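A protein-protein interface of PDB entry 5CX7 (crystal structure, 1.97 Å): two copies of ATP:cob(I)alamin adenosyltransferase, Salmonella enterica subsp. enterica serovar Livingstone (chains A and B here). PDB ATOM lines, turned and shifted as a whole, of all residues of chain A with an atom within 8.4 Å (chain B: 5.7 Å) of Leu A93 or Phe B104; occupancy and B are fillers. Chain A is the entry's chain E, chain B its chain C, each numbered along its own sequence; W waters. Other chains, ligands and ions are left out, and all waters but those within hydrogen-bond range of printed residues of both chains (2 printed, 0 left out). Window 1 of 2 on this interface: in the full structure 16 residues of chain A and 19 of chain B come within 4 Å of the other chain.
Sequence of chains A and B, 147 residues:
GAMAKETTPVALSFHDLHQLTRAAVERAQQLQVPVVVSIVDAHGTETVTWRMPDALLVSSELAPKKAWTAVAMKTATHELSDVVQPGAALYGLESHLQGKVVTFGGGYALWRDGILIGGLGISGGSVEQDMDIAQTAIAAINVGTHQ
OG1 of Thr B103 is in hydrogen-bond range of NE2 of His A96, 3.4 Å away.
The backbone carbonyl oxygen of Leu A97 is in hydrogen-bond range of the side-chain amino group of Lys A100 (3.1 Å).
The backbone carbonyl oxygen of Phe B104 is in hydrogen-bond range of the side-chain hydroxyl of Thr B77, at 2.6 Å.
The side-chain hydroxyl of Ser B81 sits at hydrogen-bond distance from the backbone carbonyl oxygen of Thr B103 (2.7 Å).
O of Val A83 lies within hydrogen-bond range of N of Ala A89, at 3.5 Å.
The backbone carbonyl oxygen (O) of Val A83 is in hydrogen-bond range of the backbone NH (N) of Leu A90.
The backbone carbonyl oxygen (O) of Gly A92 lies within hydrogen-bond range of a ring nitrogen (ND1) of His A96, 3.2 Å away.
Ala A89 touches Phe B104 (O to CB, 3.3 Å).
Leu A90 touches Phe B104 (CD2 to CE1, 3.8 Å).
Leu A90 touches Val B127 (CD2 to CG2, 3.8 Å).
O of Tyr A91 touches OG1 of Thr B103, at 3.8 Å.
CD2 of Phe B104 touches O of Tyr A91, 3.98 Å away.
Leu A93 touches Phe B104.
His A96 touches Val B102 (CD2 to CA, 3.8 Å).
His A96 touches Phe B104 (ND1 to CE2, 3.4 Å).
CD2 of Leu A97 touches CD2 of Leu B62, at 3.8 Å.
Leu A93 touches one residue of chain B.
Of the printed residues of chain A, Phe B104 touches Ala A89 (3.3 Å), Leu A90 (3.8 Å), Tyr A91 (3.98 Å), Leu A93 (3.9 Å) and His A96 (3.4 Å).
Of the printed residues of chain B, Leu A97 touches Leu B62 (3.8 Å).
Of the printed residues of chain B, His A96 touches Val B102, Thr B103 and Phe B104.
The nearest residue of chain B that does not touch Leu A93 is Leu B62 (4.2 Å).
The nearest printed residue of chain A that does not touch Phe B104 is Gly A92 (5.5 Å).
Along chain A the printed residues that touch a printed residue of chain B span positions 89 to 97.
Printed residues of chain B that touch a printed residue of chain A: Leu B62, Val B102, Thr B103, Phe B104 and Val B127.
Hydrophobic or aromatic side chains of chain B within 4 Å of the printed part of chain A: Leu B62, Val B102, Phe B104 and Val B127.
Among the printed residues, no Asp or Glu carboxylate lies within 4 Å of a Lys or Arg side-chain nitrogen of the other chain.
2 positions are printed for both chains.
Water W1 lies within hydrogen-bond range of OG1 of Thr B103 (2.4 Å) and NE2 of His A96 (3.1 Å).
Water W2 bridges the backbone carbonyl oxygen (O) of Tyr A91 (2.7 Å) and the side-chain hydroxyl (OG1) of Thr B103 (2.8 Å).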
ATOM      1  N   THR A  69      22.895  11.105  -5.319  1.00  0.00           N
ATOM      2  CA  THR A  69      24.072  10.293  -5.027  1.00  0.00           C
ATOM      3  C   THR A  69      25.340  11.158  -4.899  1.00  0.00           C
ATOM      4  O   THR A  69      26.177  10.921  -4.045  1.00  0.00           O
ATOM      5  CB  THR A  69      24.268   9.252  -6.144  1.00  0.00           C
ATOM      6  OG1 THR A  69      23.134   8.372  -6.238  1.00  0.00           O
ATOM      7  CG2 THR A  69      25.475   8.420  -5.909  1.00  0.00           C
ATOM      8  N   MET A  73      27.173  10.934  -1.366  1.00  0.00           N
ATOM      9  CA  MET A  73      28.470  10.336  -1.338  1.00  0.00           C
ATOM     10  C   MET A  73      29.661  11.293  -1.671  1.00  0.00           C
ATOM     11  O   MET A  73      30.791  10.807  -1.710  1.00  0.00           O
ATOM     12  CB  MET A  73      28.503   9.163  -2.277  1.00  0.00           C
ATOM     13  CG  MET A  73      27.365   8.241  -1.855  1.00  0.00           C
ATOM     14  SD  MET A  73      27.601   6.551  -2.057  1.00  0.00           S
ATOM     15  CE  MET A  73      29.042   6.255  -1.060  1.00  0.00           C
ATOM     16  N   THR A  75      30.709  12.633  -4.416  1.00  0.00           N
ATOM     17  CA  THR A  75      31.460  12.053  -5.484  1.00  0.00           C
ATOM     18  C   THR A  75      30.741  12.224  -6.815  1.00  0.00           C
ATOM     19  O   THR A  75      29.566  12.500  -6.832  1.00  0.00           O
ATOM     20  CB  THR A  75      31.655  10.534  -5.223  1.00  0.00           C
ATOM     21  OG1 THR A  75      32.573  10.004  -6.166  1.00  0.00           O
ATOM     22  CG2 THR A  75      30.363   9.827  -5.326  1.00  0.00           C
ATOM     23  N   LEU A  80      31.916   5.841  -8.632  1.00  0.00           N
ATOM     24  CA  LEU A  80      31.435   4.687  -7.865  1.00  0.00           C
ATOM     25  C   LEU A  80      31.451   3.364  -8.622  1.00  0.00           C
ATOM     26  O   LEU A  80      31.257   2.345  -8.012  1.00  0.00           O
ATOM     27  CB  LEU A  80      30.042   5.017  -7.360  1.00  0.00           C
ATOM     28  CG  LEU A  80      29.855   6.198  -6.425  1.00  0.00           C
ATOM     29  CD1 LEU A  80      28.378   6.407  -6.127  1.00  0.00           C
ATOM     30  CD2 LEU A  80      30.662   6.053  -5.144  1.00  0.00           C
ATOM     31  N   VAL A  83      33.961   0.665  -7.450  1.00  0.00           N
ATOM     32  CA  VAL A  83      33.945   0.311  -6.002  1.00  0.00           C
ATOM     33  C   VAL A  83      32.730  -0.524  -5.598  1.00  0.00           C
ATOM     34  O   VAL A  83      32.683  -1.170  -4.534  1.00  0.00           O
ATOM     35  CB  VAL A  83      34.131   1.575  -5.125  1.00  0.00           C
ATOM     36  CG1 VAL A  83      32.847   2.384  -4.964  1.00  0.00           C
ATOM     37  CG2 VAL A  83      34.698   1.249  -3.753  1.00  0.00           C
ATOM     38  N   VAL A  84      31.739  -0.590  -6.467  1.00  0.00           N
ATOM     39  CA  VAL A  84      30.539  -1.460  -6.205  1.00  0.00           C
ATOM     40  C   VAL A  84      30.551  -2.788  -6.958  1.00  0.00           C
ATOM     41  O   VAL A  84      29.605  -3.595  -6.861  1.00  0.00           O
ATOM     42  CB  VAL A  84      29.227  -0.710  -6.485  1.00  0.00           C
ATOM     43  CG1 VAL A  84      29.148   0.531  -5.635  1.00  0.00           C
ATOM     44  CG2 VAL A  84      29.028  -0.406  -7.978  1.00  0.00           C
ATOM     45  N   GLN A  85      31.605  -3.070  -7.727  1.00  0.00           N
ATOM     46  CA  GLN A  85      31.682  -4.306  -8.463  1.00  0.00           C
ATOM     47  C   GLN A  85      31.821  -5.514  -7.495  1.00  0.00           C
ATOM     48  O   GLN A  85      32.290  -5.334  -6.368  1.00  0.00           O
ATOM     49  CB  GLN A  85      32.903  -4.322  -9.420  1.00  0.00           C
ATOM     50  CG  GLN A  85      32.822  -3.236 -10.503  1.00  0.00           C
ATOM     51  CD  GLN A  85      31.603  -3.379 -11.363  1.00  0.00           C
ATOM     52  OE1 GLN A  85      31.379  -4.438 -11.947  1.00  0.00           O
ATOM     53  NE2 GLN A  85      30.847  -2.326 -11.490  1.00  0.00           N
ATOM     54  N   ALA A  88      34.808  -5.775  -4.886  1.00  0.00           N
ATOM     55  CA  ALA A  88      35.229  -4.455  -4.488  1.00  0.00           C
ATOM     56  C   ALA A  88      34.576  -4.013  -3.193  1.00  0.00           C
ATOM     57  O   ALA A  88      33.717  -4.697  -2.626  1.00  0.00           O
ATOM     58  CB  ALA A  88      34.919  -3.436  -5.606  1.00  0.00           C
ATOM     59  N   ALA A  89      35.067  -2.914  -2.657  1.00  0.00           N
ATOM     60  CA  ALA A  89      34.867  -2.585  -1.230  1.00  0.00           C
ATOM     61  C   ALA A  89      33.380  -2.347  -0.825  1.00  0.00           C
ATOM     62  O   ALA A  89      32.978  -2.705   0.292  1.00  0.00           O
ATOM     63  CB  ALA A  89      35.726  -1.404  -0.808  1.00  0.00           C
ATOM     64  N   LEU A  90      32.592  -1.758  -1.745  1.00  0.00           N
ATOM     65  CA  LEU A  90      31.231  -1.444  -1.545  1.00  0.00           C
ATOM     66  C   LEU A  90      30.276  -2.238  -2.436  1.00  0.00           C
ATOM     67  O   LEU A  90      29.148  -1.793  -2.716  1.00  0.00           O
ATOM     68  CB  LEU A  90      30.988   0.077  -1.719  1.00  0.00           C
ATOM     69  CG  LEU A  90      31.835   0.984  -0.842  1.00  0.00           C
ATOM     70  CD1 LEU A  90      31.507   2.443  -1.174  1.00  0.00           C
ATOM     71  CD2 LEU A  90      31.646   0.718   0.654  1.00  0.00           C
ATOM     72  N   TYR A  91      30.663  -3.452  -2.778  1.00  0.00           N
ATOM     73  CA  TYR A  91      29.711  -4.385  -3.397  1.00  0.00           C
ATOM     74  C   TYR A  91      28.363  -4.421  -2.611  1.00  0.00           C
ATOM     75  O   TYR A  91      28.333  -4.529  -1.386  1.00  0.00           O
ATOM     76  CB  TYR A  91      30.316  -5.796  -3.485  1.00  0.00           C
ATOM     77  CG  TYR A  91      29.328  -6.785  -4.017  1.00  0.00           C
ATOM     78  CD1 TYR A  91      28.988  -6.806  -5.340  1.00  0.00           C
ATOM     79  CD2 TYR A  91      28.695  -7.696  -3.146  1.00  0.00           C
ATOM     80  CE1 TYR A  91      28.038  -7.669  -5.844  1.00  0.00           C
ATOM     81  CE2 TYR A  91      27.697  -8.546  -3.623  1.00  0.00           C
ATOM     82  CZ  TYR A  91      27.398  -8.560  -4.962  1.00  0.00           C
ATOM     83  OH  TYR A  91      26.425  -9.396  -5.419  1.00  0.00           O
ATOM     84  N   GLY A  92      27.258  -4.389  -3.367  1.00  0.00           N
ATOM     85  CA  GLY A  92      25.924  -4.402  -2.815  1.00  0.00           C
ATOM     86  C   GLY A  92      25.317  -3.075  -2.483  1.00  0.00           C
ATOM     87  O   GLY A  92      24.162  -3.033  -2.106  1.00  0.00           O
ATOM     88  N   LEU A  93      26.091  -1.963  -2.634  1.00  0.00           N
ATOM     89  CA  LEU A  93      25.667  -0.663  -2.130  1.00  0.00           C
ATOM     90  C   LEU A  93      24.323  -0.201  -2.657  1.00  0.00           C
ATOM     91  O   LEU A  93      23.500   0.302  -1.884  1.00  0.00           O
ATOM     92  CB  LEU A  93      26.722   0.408  -2.468  1.00  0.00           C
ATOM     93  CG  LEU A  93      26.471   1.769  -1.930  1.00  0.00           C
ATOM     94  CD1 LEU A  93      26.701   1.813  -0.418  1.00  0.00           C
ATOM     95  CD2 LEU A  93      27.407   2.758  -2.632  1.00  0.00           C
ATOM     96  N   GLU A  94      24.084  -0.473  -3.933  1.00  0.00           N
ATOM     97  CA  GLU A  94      22.852  -0.081  -4.594  1.00  0.00           C
ATOM     98  C   GLU A  94      21.625  -0.743  -3.932  1.00  0.00           C
ATOM     99  O   GLU A  94      20.546  -0.130  -3.861  1.00  0.00           O
ATOM    100  CB  GLU A  94      22.863  -0.308  -6.082  1.00  0.00           C
ATOM    101  CG  GLU A  94      22.911  -1.731  -6.627  1.00  0.00           C
ATOM    102  CD  GLU A  94      24.233  -2.472  -6.457  1.00  0.00           C
ATOM    103  OE1 GLU A  94      25.281  -1.865  -6.178  1.00  0.00           O
ATOM    104  OE2 GLU A  94      24.170  -3.725  -6.484  1.00  0.00           O
ATOM    105  N   SER A  95      21.779  -1.972  -3.453  1.00  0.00           N
ATOM    106  CA  SER A  95      20.653  -2.636  -2.743  1.00  0.00           C
ATOM    107  C   SER A  95      20.580  -2.193  -1.287  1.00  0.00           C
ATOM    108  O   SER A  95      19.476  -2.025  -0.705  1.00  0.00           O
ATOM    109  CB  SER A  95      20.862  -4.113  -2.760  1.00  0.00           C
ATOM    110  OG  SER A  95      20.752  -4.589  -4.047  1.00  0.00           O
ATOM    111  N   HIS A  96      21.737  -1.989  -0.654  1.00  0.00           N
ATOM    112  CA  HIS A  96      21.732  -1.500   0.719  1.00  0.00           C
ATOM    113  C   HIS A  96      20.962  -0.199   0.883  1.00  0.00           C
ATOM    114  O   HIS A  96      20.408   0.031   1.968  1.00  0.00           O
ATOM    115  CB  HIS A  96      23.130  -1.282   1.260  1.00  0.00           C
ATOM    116  CG  HIS A  96      24.012  -2.451   1.086  1.00  0.00           C
ATOM    117  ND1 HIS A  96      25.359  -2.339   0.828  1.00  0.00           N
ATOM    118  CD2 HIS A  96      23.752  -3.780   1.149  1.00  0.00           C
ATOM    119  CE1 HIS A  96      25.905  -3.543   0.773  1.00  0.00           C
ATOM    120  NE2 HIS A  96      24.935  -4.430   0.912  1.00  0.00           N
ATOM    121  N   LEU A  97      21.075   0.706  -0.116  1.00  0.00           N
ATOM    122  CA  LEU A  97      20.456   1.963  -0.023  1.00  0.00           C
ATOM    123  C   LEU A  97      19.122   1.960  -0.818  1.00  0.00           C
ATOM    124  O   LEU A  97      18.607   3.042  -1.113  1.00  0.00           O
ATOM    125  CB  LEU A  97      21.439   3.030  -0.528  1.00  0.00           C
ATOM    126  CG  LEU A  97      22.640   3.187   0.410  1.00  0.00           C
ATOM    127  CD1 LEU A  97      23.641   4.099  -0.229  1.00  0.00           C
ATOM    128  CD2 LEU A  97      22.193   3.744   1.760  1.00  0.00           C
ATOM    129  N   GLN A  98      18.570   0.791  -1.082  1.00  0.00           N
ATOM    130  CA  GLN A  98      17.185   0.606  -1.634  1.00  0.00           C
ATOM    131  C   GLN A  98      17.006   1.377  -2.940  1.00  0.00           C
ATOM    132  O   GLN A  98      15.972   2.018  -3.155  1.00  0.00           O
ATOM    133  CB  GLN A  98      16.112   1.053  -0.618  1.00  0.00           C
ATOM    134  CG  GLN A  98      16.269   0.530   0.814  1.00  0.00           C
ATOM    135  CD  GLN A  98      15.282   1.200   1.779  1.00  0.00           C
ATOM    136  OE1 GLN A  98      14.101   0.923   1.751  1.00  0.00           O
ATOM    137  NE2 GLN A  98      15.795   2.089   2.650  1.00  0.00           N
ATOM    138  N   GLY A  99      18.045   1.361  -3.762  1.00  0.00           N
ATOM    139  CA  GLY A  99      17.964   2.018  -5.049  1.00  0.00           C
ATOM    140  C   GLY A  99      18.165   3.514  -5.058  1.00  0.00           C
ATOM    141  O   GLY A  99      18.048   4.117  -6.113  1.00  0.00           O
ATOM    142  N   LYS A 100      18.511   4.130  -3.919  1.00  0.00           N
ATOM    143  CA  LYS A 100      18.658   5.589  -3.895  1.00  0.00           C
ATOM    144  C   LYS A 100      19.939   6.083  -4.560  1.00  0.00           C
ATOM    145  O   LYS A 100      20.007   7.256  -4.951  1.00  0.00           O
ATOM    146  CB  LYS A 100      18.612   6.121  -2.488  1.00  0.00           C
ATOM    147  CG  LYS A 100      17.184   6.040  -1.948  1.00  0.00           C
ATOM    148  CD  LYS A 100      17.025   6.887  -0.726  1.00  0.00           C
ATOM    149  CE  LYS A 100      17.841   6.352   0.408  1.00  0.00           C
ATOM    150  NZ  LYS A 100      17.251   5.069   0.851  1.00  0.00           N
ATOM    151  N   VAL A 101      20.938   5.232  -4.663  1.00  0.00           N
ATOM    152  CA  VAL A 101      22.212   5.585  -5.255  1.00  0.00           C
ATOM    153  C   VAL A 101      22.330   4.937  -6.646  1.00  0.00           C
ATOM    154  O   VAL A 101      21.923   3.791  -6.837  1.00  0.00           O
ATOM    155  CB  VAL A 101      23.455   5.254  -4.434  1.00  0.00           C
ATOM    156  CG1 VAL A 101      23.442   6.094  -3.148  1.00  0.00           C
ATOM    157  CG2 VAL A 101      23.608   3.779  -4.190  1.00  0.00           C
ATOM    158  N   VAL A 102      22.878   5.711  -7.605  1.00  0.00           N
ATOM    159  CA  VAL A 102      23.171   5.228  -8.933  1.00  0.00           C
ATOM    160  C   VAL A 102      24.656   5.281  -9.098  1.00  0.00           C
ATOM    161  O   VAL A 102      25.280   6.320  -8.782  1.00  0.00           O
ATOM    162  CB  VAL A 102      22.421   6.078 -10.006  1.00  0.00           C
ATOM    163  CG1 VAL A 102      22.908   5.704 -11.400  1.00  0.00           C
ATOM    164  CG2 VAL A 102      20.907   5.872  -9.917  1.00  0.00           C
ATOM    165  N   THR A 103      25.227   4.223  -9.627  1.00  0.00           N
ATOM    166  CA  THR A 103      26.671   4.011  -9.615  1.00  0.00           C
ATOM    167  C   THR A 103      27.323   3.998 -10.979  1.00  0.00           C
ATOM    168  O   THR A 103      28.481   3.567 -11.149  1.00  0.00           O
ATOM    169  CB  THR A 103      26.979   2.702  -8.882  1.00  0.00           C
ATOM    170  OG1 THR A 103      26.237   1.630  -9.487  1.00  0.00           O
ATOM    171  CG2 THR A 103      26.512   2.831  -7.425  1.00  0.00           C
ATOM    172  N   LEU B  62      23.291   3.752   6.325  1.00  0.00           N
ATOM    173  CA  LEU B  62      24.236   2.627   6.456  1.00  0.00           C
ATOM    174  C   LEU B  62      24.659   2.252   7.891  1.00  0.00           C
ATOM    175  O   LEU B  62      24.782   1.069   8.188  1.00  0.00           O
ATOM    176  CB  LEU B  62      25.538   2.871   5.646  1.00  0.00           C
ATOM    177  CG  LEU B  62      25.359   2.977   4.107  1.00  0.00           C
ATOM    178  CD1 LEU B  62      26.650   3.416   3.472  1.00  0.00           C
ATOM    179  CD2 LEU B  62      24.895   1.660   3.476  1.00  0.00           C
ATOM    180  N   LYS B  66      24.221  -1.410   9.418  1.00  0.00           N
ATOM    181  CA  LYS B  66      25.362  -2.247   9.811  1.00  0.00           C
ATOM    182  C   LYS B  66      25.173  -2.812  11.235  1.00  0.00           C
ATOM    183  O   LYS B  66      25.430  -3.998  11.509  1.00  0.00           O
ATOM    184  CB  LYS B  66      26.671  -1.488   9.773  1.00  0.00           C
ATOM    185  CG  LYS B  66      27.144  -1.220   8.359  1.00  0.00           C
ATOM    186  CD  LYS B  66      28.463  -0.499   8.391  1.00  0.00           C
ATOM    187  CE  LYS B  66      28.817   0.128   7.082  1.00  0.00           C
ATOM    188  NZ  LYS B  66      30.119   0.845   7.137  1.00  0.00           N
ATOM    189  N   THR B  77      29.982  -7.245  10.010  1.00  0.00           N
ATOM    190  CA  THR B  77      29.484  -7.080   8.614  1.00  0.00           C
ATOM    191  C   THR B  77      30.598  -7.381   7.619  1.00  0.00           C
ATOM    192  O   THR B  77      30.296  -7.860   6.566  1.00  0.00           O
ATOM    193  CB  THR B  77      28.854  -5.736   8.382  1.00  0.00           C
ATOM    194  OG1 THR B  77      29.798  -4.679   8.660  1.00  0.00           O
ATOM    195  CG2 THR B  77      27.598  -5.565   9.253  1.00  0.00           C
ATOM    196  N   HIS B  78      31.880  -7.164   8.002  1.00  0.00           N
ATOM    197  CA  HIS B  78      32.995  -7.523   7.094  1.00  0.00           C
ATOM    198  C   HIS B  78      33.084  -9.025   6.852  1.00  0.00           C
ATOM    199  O   HIS B  78      33.603  -9.459   5.820  1.00  0.00           O
ATOM    200  CB  HIS B  78      34.314  -6.949   7.547  1.00  0.00           C
ATOM    201  CG  HIS B  78      34.868  -7.610   8.781  1.00  0.00           C
ATOM    202  ND1 HIS B  78      34.515  -7.246  10.070  1.00  0.00           N
ATOM    203  CD2 HIS B  78      35.765  -8.611   8.910  1.00  0.00           C
ATOM    204  CE1 HIS B  78      35.200  -7.976  10.936  1.00  0.00           C
ATOM    205  NE2 HIS B  78      35.924  -8.850  10.261  1.00  0.00           N
ATOM    206  N   SER B  81      31.165 -10.144   3.643  1.00  0.00           N
ATOM    207  CA  SER B  81      31.593  -9.778   2.298  1.00  0.00           C
ATOM    208  C   SER B  81      31.826 -10.936   1.391  1.00  0.00           C
ATOM    209  O   SER B  81      31.379 -10.924   0.236  1.00  0.00           O
ATOM    210  CB  SER B  81      32.873  -8.902   2.330  1.00  0.00           C
ATOM    211  OG  SER B  81      32.606  -7.877   3.282  1.00  0.00           O
ATOM    212  N   VAL B 102      23.759  -4.851   5.389  1.00  0.00           N
ATOM    213  CA  VAL B 102      24.963  -4.262   4.748  1.00  0.00           C
ATOM    214  C   VAL B 102      26.081  -5.238   4.959  1.00  0.00           C
ATOM    215  O   VAL B 102      26.300  -5.791   6.068  1.00  0.00           O
ATOM    216  CB  VAL B 102      25.267  -2.894   5.356  1.00  0.00           C
ATOM    217  CG1 VAL B 102      26.639  -2.403   4.887  1.00  0.00           C
ATOM    218  CG2 VAL B 102      24.189  -1.896   5.014  1.00  0.00           C
ATOM    219  N   THR B 103      26.811  -5.530   3.897  1.00  0.00           N
ATOM    220  CA  THR B 103      27.731  -6.636   3.815  1.00  0.00           C
ATOM    221  C   THR B 103      29.206  -6.231   3.648  1.00  0.00           C
ATOM    222  O   THR B 103      30.054  -7.078   3.307  1.00  0.00           O
ATOM    223  CB  THR B 103      27.286  -7.606   2.663  1.00  0.00           C
ATOM    224  OG1 THR B 103      27.212  -6.859   1.458  1.00  0.00           O
ATOM    225  CG2 THR B 103      25.893  -8.151   2.988  1.00  0.00           C
ATOM    226  N   PHE B 104      29.505  -4.967   3.938  1.00  0.00           N
ATOM    227  CA  PHE B 104      30.853  -4.500   4.070  1.00  0.00           C
ATOM    228  C   PHE B 104      31.095  -4.018   5.457  1.00  0.00           C
ATOM    229  O   PHE B 104      30.152  -3.772   6.225  1.00  0.00           O
ATOM    230  CB  PHE B 104      31.241  -3.452   2.978  1.00  0.00           C
ATOM    231  CG  PHE B 104      30.245  -2.310   2.804  1.00  0.00           C
ATOM    232  CD1 PHE B 104      30.248  -1.241   3.683  1.00  0.00           C
ATOM    233  CD2 PHE B 104      29.339  -2.327   1.776  1.00  0.00           C
ATOM    234  CE1 PHE B 104      29.383  -0.180   3.521  1.00  0.00           C
ATOM    235  CE2 PHE B 104      28.492  -1.237   1.562  1.00  0.00           C
ATOM    236  CZ  PHE B 104      28.445  -0.211   2.479  1.00  0.00           C
ATOM    237  N   GLY B 105      32.354  -3.894   5.818  1.00  0.00           N
ATOM    238  CA  GLY B 105      32.759  -3.609   7.201  1.00  0.00           C
ATOM    239  C   GLY B 105      32.241  -2.337   7.867  1.00  0.00           C
ATOM    240  O   GLY B 105      31.947  -1.327   7.209  1.00  0.00           O
ATOM    241  N   GLY B 106      32.206  -2.404   9.197  1.00  0.00           N
ATOM    242  CA  GLY B 106      31.836  -1.326  10.010  1.00  0.00           C
ATOM    243  C   GLY B 106      30.846  -1.675  11.099  1.00  0.00           C
ATOM    244  O   GLY B 106      30.524  -0.851  11.942  1.00  0.00           O
ATOM    245  N   GLY B 107      30.246  -2.832  10.985  1.00  0.00           N
ATOM    246  CA  GLY B 107      29.266  -3.329  11.967  1.00  0.00           C
ATOM    247  C   GLY B 107      29.892  -4.474  12.733  1.00  0.00           C
ATOM    248  O   GLY B 107      30.472  -5.370  12.129  1.00  0.00           O
ATOM    249  N   VAL B 127      35.822   2.000   4.397  1.00  0.00           N
ATOM    250  CA  VAL B 127      35.471   0.798   5.145  1.00  0.00           C
ATOM    251  C   VAL B 127      36.509   0.558   6.257  1.00  0.00           C
ATOM    252  O   VAL B 127      36.137   0.196   7.395  1.00  0.00           O
ATOM    253  CB  VAL B 127      35.363  -0.430   4.228  1.00  0.00           C
ATOM    254  CG1 VAL B 127      35.190  -1.720   5.066  1.00  0.00           C
ATOM    255  CG2 VAL B 127      34.175  -0.268   3.272  1.00  0.00           C
ATOM    256  N   ASP B 130      35.969   2.961   9.110  1.00  0.00           N
ATOM    257  CA  ASP B 130      34.753   2.626   9.865  1.00  0.00           C
ATOM    258  C   ASP B 130      35.087   1.503  10.857  1.00  0.00           C
ATOM    259  O   ASP B 130      34.566   1.462  11.968  1.00  0.00           O
ATOM    260  CB  ASP B 130      33.626   2.180   8.910  1.00  0.00           C
ATOM    261  CG  ASP B 130      33.040   3.313   8.040  1.00  0.00           C
ATOM    262  OD1 ASP B 130      33.214   4.520   8.321  1.00  0.00           O
ATOM    263  OD2 ASP B 130      32.331   2.956   7.042  1.00  0.00           O
HETATM  264  O   HOH W   1      25.623  -7.134  -0.338  1.00  0.00           O
HETATM  265  O   HOH W   2      29.646  -6.066   0.382  1.00  0.00           O
